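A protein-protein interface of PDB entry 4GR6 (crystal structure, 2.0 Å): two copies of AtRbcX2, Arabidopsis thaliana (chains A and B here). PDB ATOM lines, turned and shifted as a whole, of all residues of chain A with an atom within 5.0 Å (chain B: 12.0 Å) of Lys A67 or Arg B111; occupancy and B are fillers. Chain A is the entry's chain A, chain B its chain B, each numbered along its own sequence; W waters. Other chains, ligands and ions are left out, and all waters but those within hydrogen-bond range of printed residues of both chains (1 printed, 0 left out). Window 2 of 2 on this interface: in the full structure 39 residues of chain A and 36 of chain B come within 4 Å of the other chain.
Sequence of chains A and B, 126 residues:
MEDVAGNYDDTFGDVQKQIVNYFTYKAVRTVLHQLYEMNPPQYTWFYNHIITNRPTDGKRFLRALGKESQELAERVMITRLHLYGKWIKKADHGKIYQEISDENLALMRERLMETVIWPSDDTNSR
Water W1 lies within hydrogen-bond range of O of Arg A63 (2.6 Å) and NH1 of Arg B111 (3.1 Å).
The guanidinium group (NE) of Arg A63 lies within salt-bridge range of the side-chain carboxylate (OE1) of Glu B110, at 2.7 Å. The side-chain amide nitrogen (NE2) of Gln A70 is in hydrogen-bond range of the side-chain sulfur (SD) of Met B108 (3.0 Å).
Of the 14 printed residues of chain B, 4 touch a printed residue of chain A. Hydrophobic or aromatic side chains of chain B within 4 Å of the printed part of chain A: Leu B107 and Met B108. Along chain A the printed residues that touch a printed residue of chain B span positions 63 to 70. Among the printed residues, 6 pairs touch across the chains.
No position is printed for both chains. Of the 6 pairs that touch across the chains among the printed residues, none has its exchanged pair printed and touching as well.
Of the printed residues of chain B, Arg A63 touches Leu B107 and Glu B110. No residue of chain B comes within 4 Å of Ala A64. No residue of chain B comes within 4 Å of Leu A65. Printed residues of chain B within 4 Å of Gly A66: Arg B111. Of chain B, only Arg B111 comes within 4 Å of Lys A67. No residue of chain B comes within 4 Å of Glu A68. Gln A70 touches just these residues of chain B: Met B108 and Arg B111. Asn B104 touches none of the printed residues of chain A. Leu B105 touches none of the printed residues of chain A. Of the printed residues of chain A, Met B108 touches Gln A70 (3.0 Å). Of the printed residues of chain A, Glu B110 touches Arg A63. Of chain A, only Gly A66 (3.5 Å), Lys A67 (3.6 Å) and Gln A70 (3.1 Å) come within 4 Å of Arg B111. The nearest residue of chain B that does not touch Lys A67 is Glu B114 (5.6 Å). The nearest printed residue of chain A that does not touch Arg B111 is Arg A63 (5.0 Å). The nearest printed residue of chain A that does not touch Glu B110 is Lys A67 (6.5 Å).
Among the printed residues, merely in contact across the chains: Arg A63 with Leu B107 (3.6 Å), Gly A66 with Arg B111 (3.5 Å), Lys A67 with Arg B111 (3.6 Å) and Gln A70 with Arg B111 (3.1 Å).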
ATOM      1  N   ARG A  63       1.270   5.448  -1.200  1.00  0.00           N
ATOM      2  CA  ARG A  63       1.470   5.894   0.182  1.00  0.00           C
ATOM      3  C   ARG A  63       2.834   5.453   0.709  1.00  0.00           C
ATOM      4  O   ARG A  63       3.610   6.223   1.315  1.00  0.00           O
ATOM      5  CB  ARG A  63       0.389   5.314   1.115  1.00  0.00           C
ATOM      6  CG  ARG A  63      -0.959   5.853   0.981  1.00  0.00           C
ATOM      7  CD  ARG A  63      -1.748   5.498   2.251  1.00  0.00           C
ATOM      8  NE  ARG A  63      -2.978   6.248   2.284  1.00  0.00           N
ATOM      9  CZ  ARG A  63      -4.177   5.741   2.039  1.00  0.00           C
ATOM     10  NH1 ARG A  63      -4.328   4.454   1.752  1.00  0.00           N
ATOM     11  NH2 ARG A  63      -5.229   6.533   2.095  1.00  0.00           N
ATOM     12  N   ALA A  64       3.134   4.188   0.501  1.00  0.00           N
ATOM     13  CA  ALA A  64       4.389   3.642   0.999  1.00  0.00           C
ATOM     14  C   ALA A  64       5.578   4.237   0.239  1.00  0.00           C
ATOM     15  O   ALA A  64       6.632   4.541   0.842  1.00  0.00           O
ATOM     16  CB  ALA A  64       4.378   2.119   0.890  1.00  0.00           C
ATOM     17  N   LEU A  65       5.433   4.419  -1.072  1.00  0.00           N
ATOM     18  CA  LEU A  65       6.547   5.017  -1.838  1.00  0.00           C
ATOM     19  C   LEU A  65       6.804   6.437  -1.353  1.00  0.00           C
ATOM     20  O   LEU A  65       7.945   6.883  -1.213  1.00  0.00           O
ATOM     21  CB  LEU A  65       6.235   5.033  -3.347  1.00  0.00           C
ATOM     22  CG  LEU A  65       7.233   5.817  -4.230  1.00  0.00           C
ATOM     23  CD1 LEU A  65       8.656   5.331  -4.030  1.00  0.00           C
ATOM     24  CD2 LEU A  65       6.823   5.662  -5.691  1.00  0.00           C
ATOM     25  N   GLY A  66       5.720   7.158  -1.112  1.00  0.00           N
ATOM     26  CA  GLY A  66       5.801   8.526  -0.666  1.00  0.00           C
ATOM     27  C   GLY A  66       6.532   8.709   0.652  1.00  0.00           C
ATOM     28  O   GLY A  66       7.149   9.759   0.880  1.00  0.00           O
ATOM     29  N   LYS A  67       6.489   7.700   1.524  1.00  0.00           N
ATOM     30  CA  LYS A  67       7.208   7.807   2.779  1.00  0.00           C
ATOM     31  C   LYS A  67       8.736   7.839   2.589  1.00  0.00           C
ATOM     32  O   LYS A  67       9.466   8.292   3.472  1.00  0.00           O
ATOM     33  CB  LYS A  67       6.813   6.656   3.702  1.00  0.00           C
ATOM     34  CG  LYS A  67       5.417   6.781   4.268  1.00  0.00           C
ATOM     35  CD  LYS A  67       5.112   5.569   5.158  1.00  0.00           C
ATOM     36  CE  LYS A  67       3.984   5.856   6.163  1.00  0.00           C
ATOM     37  NZ  LYS A  67       2.637   5.913   5.541  1.00  0.00           N
ATOM     38  N   GLU A  68       9.211   7.368   1.436  1.00  0.00           N
ATOM     39  CA  GLU A  68      10.663   7.251   1.184  1.00  0.00           C
ATOM     40  C   GLU A  68      11.157   8.158   0.087  1.00  0.00           C
ATOM     41  O   GLU A  68      12.308   8.584   0.105  1.00  0.00           O
ATOM     42  CB  GLU A  68      11.042   5.794   0.822  1.00  0.00           C
ATOM     43  CG  GLU A  68      10.765   4.815   1.930  1.00  0.00           C
ATOM     44  CD  GLU A  68      11.398   3.445   1.689  1.00  0.00           C
ATOM     45  OE1 GLU A  68      12.646   3.328   1.595  1.00  0.00           O
ATOM     46  OE2 GLU A  68      10.617   2.490   1.588  1.00  0.00           O
ATOM     47  N   SER A  69      10.290   8.459  -0.871  1.00  0.00           N
ATOM     48  CA  SER A  69      10.648   9.346  -1.963  1.00  0.00           C
ATOM     49  C   SER A  69       9.398   9.991  -2.521  1.00  0.00           C
ATOM     50  O   SER A  69       8.704   9.444  -3.384  1.00  0.00           O
ATOM     51  CB  SER A  69      11.401   8.592  -3.069  1.00  0.00           C
ATOM     52  OG  SER A  69      11.672   9.470  -4.154  1.00  0.00           O
ATOM     53  N   GLN A  70       9.083  11.165  -2.012  1.00  0.00           N
ATOM     54  CA  GLN A  70       7.925  11.899  -2.524  1.00  0.00           C
ATOM     55  C   GLN A  70       8.083  12.317  -3.996  1.00  0.00           C
ATOM     56  O   GLN A  70       7.087  12.441  -4.715  1.00  0.00           O
ATOM     57  CB  GLN A  70       7.669  13.120  -1.629  1.00  0.00           C
ATOM     58  CG  GLN A  70       6.242  13.733  -1.734  1.00  0.00           C
ATOM     59  CD  GLN A  70       5.127  12.770  -2.194  1.00  0.00           C
ATOM     60  OE1 GLN A  70       4.720  11.837  -1.480  1.00  0.00           O
ATOM     61  NE2 GLN A  70       4.593  13.039  -3.380  1.00  0.00           N
ATOM     62  N   ASP B 102      -8.044  13.635  -8.203  1.00  0.00           N
ATOM     63  CA  ASP B 102      -8.466  13.881  -6.802  1.00  0.00           C
ATOM     64  C   ASP B 102      -7.618  13.043  -5.821  1.00  0.00           C
ATOM     65  O   ASP B 102      -7.123  13.532  -4.782  1.00  0.00           O
ATOM     66  CB  ASP B 102      -9.948  13.488  -6.594  1.00  0.00           C
ATOM     67  CG  ASP B 102     -10.927  14.466  -7.198  1.00  0.00           C
ATOM     68  OD1 ASP B 102     -10.539  15.620  -7.520  1.00  0.00           O
ATOM     69  OD2 ASP B 102     -12.122  14.078  -7.307  1.00  0.00           O
ATOM     70  N   GLU B 103      -7.437  11.786  -6.177  1.00  0.00           N
ATOM     71  CA  GLU B 103      -6.626  10.871  -5.348  1.00  0.00           C
ATOM     72  C   GLU B 103      -5.134  11.297  -5.293  1.00  0.00           C
ATOM     73  O   GLU B 103      -4.514  11.277  -4.226  1.00  0.00           O
ATOM     74  CB  GLU B 103      -6.781   9.430  -5.836  1.00  0.00           C
ATOM     75  CG  GLU B 103      -6.092   8.414  -4.923  1.00  0.00           C
ATOM     76  CD  GLU B 103      -6.202   7.004  -5.446  1.00  0.00           C
ATOM     77  OE1 GLU B 103      -5.347   6.585  -6.249  1.00  0.00           O
ATOM     78  OE2 GLU B 103      -7.139   6.317  -5.020  1.00  0.00           O
ATOM     79  N   ASN B 104      -4.559  11.733  -6.418  1.00  0.00           N
ATOM     80  CA  ASN B 104      -3.189  12.262  -6.397  1.00  0.00           C
ATOM     81  C   ASN B 104      -3.067  13.396  -5.374  1.00  0.00           C
ATOM     82  O   ASN B 104      -2.102  13.486  -4.603  1.00  0.00           O
ATOM     83  CB  ASN B 104      -2.796  12.863  -7.771  1.00  0.00           C
ATOM     84  CG  ASN B 104      -2.555  11.815  -8.827  1.00  0.00           C
ATOM     85  OD1 ASN B 104      -2.463  10.589  -8.552  1.00  0.00           O
ATOM     86  ND2 ASN B 104      -2.430  12.283 -10.060  1.00  0.00           N
ATOM     87  N   LEU B 105      -4.022  14.307  -5.404  1.00  0.00           N
ATOM     88  CA  LEU B 105      -3.916  15.483  -4.541  1.00  0.00           C
ATOM     89  C   LEU B 105      -4.118  15.042  -3.095  1.00  0.00           C
ATOM     90  O   LEU B 105      -3.467  15.560  -2.190  1.00  0.00           O
ATOM     91  CB  LEU B 105      -4.973  16.534  -4.922  1.00  0.00           C
ATOM     92  CG  LEU B 105      -4.790  17.945  -4.372  1.00  0.00           C
ATOM     93  CD1 LEU B 105      -3.480  18.514  -4.910  1.00  0.00           C
ATOM     94  CD2 LEU B 105      -5.977  18.841  -4.785  1.00  0.00           C
ATOM     95  N   ALA B 106      -5.046  14.114  -2.882  1.00  0.00           N
ATOM     96  CA  ALA B 106      -5.287  13.566  -1.536  1.00  0.00           C
ATOM     97  C   ALA B 106      -4.037  12.862  -0.946  1.00  0.00           C
ATOM     98  O   ALA B 106      -3.749  13.000   0.250  1.00  0.00           O
ATOM     99  CB  ALA B 106      -6.458  12.620  -1.551  1.00  0.00           C
ATOM    100  N   LEU B 107      -3.293  12.125  -1.764  1.00  0.00           N
ATOM    101  CA  LEU B 107      -2.054  11.484  -1.292  1.00  0.00           C
ATOM    102  C   LEU B 107      -0.983  12.492  -0.956  1.00  0.00           C
ATOM    103  O   LEU B 107      -0.197  12.294  -0.034  1.00  0.00           O
ATOM    104  CB  LEU B 107      -1.518  10.564  -2.356  1.00  0.00           C
ATOM    105  CG  LEU B 107      -2.353   9.310  -2.493  1.00  0.00           C
ATOM    106  CD1 LEU B 107      -2.006   8.677  -3.792  1.00  0.00           C
ATOM    107  CD2 LEU B 107      -2.023   8.417  -1.319  1.00  0.00           C
ATOM    108  N   MET B 108      -0.962  13.599  -1.684  1.00  0.00           N
ATOM    109  CA  MET B 108      -0.021  14.673  -1.357  1.00  0.00           C
ATOM    110  C   MET B 108      -0.359  15.335  -0.019  1.00  0.00           C
ATOM    111  O   MET B 108       0.531  15.639   0.772  1.00  0.00           O
ATOM    112  CB  MET B 108       0.004  15.712  -2.485  1.00  0.00           C
ATOM    113  CG  MET B 108       0.955  15.329  -3.617  1.00  0.00           C
ATOM    114  SD  MET B 108       2.710  15.394  -3.145  1.00  0.00           S
ATOM    115  CE  MET B 108       2.928  17.144  -2.862  1.00  0.00           C
ATOM    116  N   ARG B 109      -1.644  15.542   0.224  1.00  0.00           N
ATOM    117  CA  ARG B 109      -2.131  16.071   1.491  1.00  0.00           C
ATOM    118  C   ARG B 109      -1.730  15.156   2.642  1.00  0.00           C
ATOM    119  O   ARG B 109      -1.296  15.626   3.683  1.00  0.00           O
ATOM    120  CB  ARG B 109      -3.659  16.229   1.436  1.00  0.00           C
ATOM    121  CG  ARG B 109      -4.374  16.409   2.793  1.00  0.00           C
ATOM    122  CD  ARG B 109      -5.883  16.408   2.622  1.00  0.00           C
ATOM    123  NE  ARG B 109      -6.409  15.077   2.370  1.00  0.00           N
ATOM    124  CZ  ARG B 109      -7.379  14.793   1.506  1.00  0.00           C
ATOM    125  NH1 ARG B 109      -7.949  15.741   0.777  1.00  0.00           N
ATOM    126  NH2 ARG B 109      -7.790  13.546   1.374  1.00  0.00           N
ATOM    127  N   GLU B 110      -1.868  13.844   2.465  1.00  0.00           N
ATOM    128  CA  GLU B 110      -1.454  12.917   3.516  1.00  0.00           C
ATOM    129  C   GLU B 110       0.003  13.177   3.899  1.00  0.00           C
ATOM    130  O   GLU B 110       0.337  13.151   5.082  1.00  0.00           O
ATOM    131  CB  GLU B 110      -1.645  11.473   3.092  1.00  0.00           C
ATOM    132  CG  GLU B 110      -3.061  11.143   2.825  1.00  0.00           C
ATOM    133  CD  GLU B 110      -3.273   9.651   2.563  1.00  0.00           C
ATOM    134  OE1 GLU B 110      -2.285   8.886   2.555  1.00  0.00           O
ATOM    135  OE2 GLU B 110      -4.434   9.249   2.381  1.00  0.00           O
ATOM    136  N   ARG B 111       0.843  13.525   2.929  1.00  0.00           N
ATOM    137  CA  ARG B 111       2.266  13.791   3.213  1.00  0.00           C
ATOM    138  C   ARG B 111       2.434  14.952   4.183  1.00  0.00           C
ATOM    139  O   ARG B 111       3.251  14.868   5.094  1.00  0.00           O
ATOM    140  CB  ARG B 111       3.064  14.077   1.935  1.00  0.00           C
ATOM    141  CG  ARG B 111       3.236  12.906   1.013  1.00  0.00           C
ATOM    142  CD  ARG B 111       3.778  11.694   1.747  1.00  0.00           C
ATOM    143  NE  ARG B 111       4.973  11.992   2.535  1.00  0.00           N
ATOM    144  CZ  ARG B 111       5.334  11.295   3.617  1.00  0.00           C
ATOM    145  NH1 ARG B 111       4.607  10.249   4.020  1.00  0.00           N
ATOM    146  NH2 ARG B 111       6.436  11.620   4.289  1.00  0.00           N
ATOM    147  N   LEU B 112       1.671  16.037   3.983  1.00  0.00           N
ATOM    148  CA  LEU B 112       1.774  17.211   4.843  1.00  0.00           C
ATOM    149  C   LEU B 112       1.389  16.847   6.267  1.00  0.00           C
ATOM    150  O   LEU B 112       1.832  17.484   7.219  1.00  0.00           O
ATOM    151  CB  LEU B 112       0.849  18.351   4.373  1.00  0.00           C
ATOM    152  CG  LEU B 112       1.221  19.238   3.180  1.00  0.00           C
ATOM    153  CD1 LEU B 112       2.573  19.932   3.397  1.00  0.00           C
ATOM    154  CD2 LEU B 112       1.215  18.464   1.900  1.00  0.00           C
ATOM    155  N   MET B 113       0.533  15.842   6.403  1.00  0.00           N
ATOM    156  CA  MET B 113       0.060  15.422   7.711  1.00  0.00           C
ATOM    157  C   MET B 113       1.211  14.831   8.513  1.00  0.00           C
ATOM    158  O   MET B 113       1.377  15.145   9.692  1.00  0.00           O
ATOM    159  CB  MET B 113      -1.094  14.428   7.585  1.00  0.00           C
ATOM    160  CG  MET B 113      -2.456  15.080   7.385  1.00  0.00           C
ATOM    161  SD  MET B 113      -2.775  16.345   8.646  1.00  0.00           S
ATOM    162  CE  MET B 113      -3.080  15.380  10.132  1.00  0.00           C
ATOM    163  N   GLU B 114       2.026  14.007   7.861  1.00  0.00           N
ATOM    164  CA  GLU B 114       3.241  13.479   8.473  1.00  0.00           C
ATOM    165  C   GLU B 114       4.294  14.580   8.534  1.00  0.00           C
ATOM    166  O   GLU B 114       5.369  14.441   7.957  1.00  0.00           O
ATOM    167  CB  GLU B 114       3.776  12.290   7.672  1.00  0.00           C
ATOM    168  CG  GLU B 114       2.763  11.162   7.464  1.00  0.00           C
ATOM    169  N   THR B 115       3.969  15.670   9.234  1.00  0.00           N
ATOM    170  CA  THR B 115       4.825  16.861   9.303  1.00  0.00           C
ATOM    171  C   THR B 115       4.687  17.593  10.647  1.00  0.00           C
ATOM    172  O   THR B 115       3.687  17.444  11.363  1.00  0.00           O
ATOM    173  CB  THR B 115       4.486  17.865   8.179  1.00  0.00           C
HETATM  174  O   HOH W   1       2.998   8.683   1.943  1.00  0.00           O
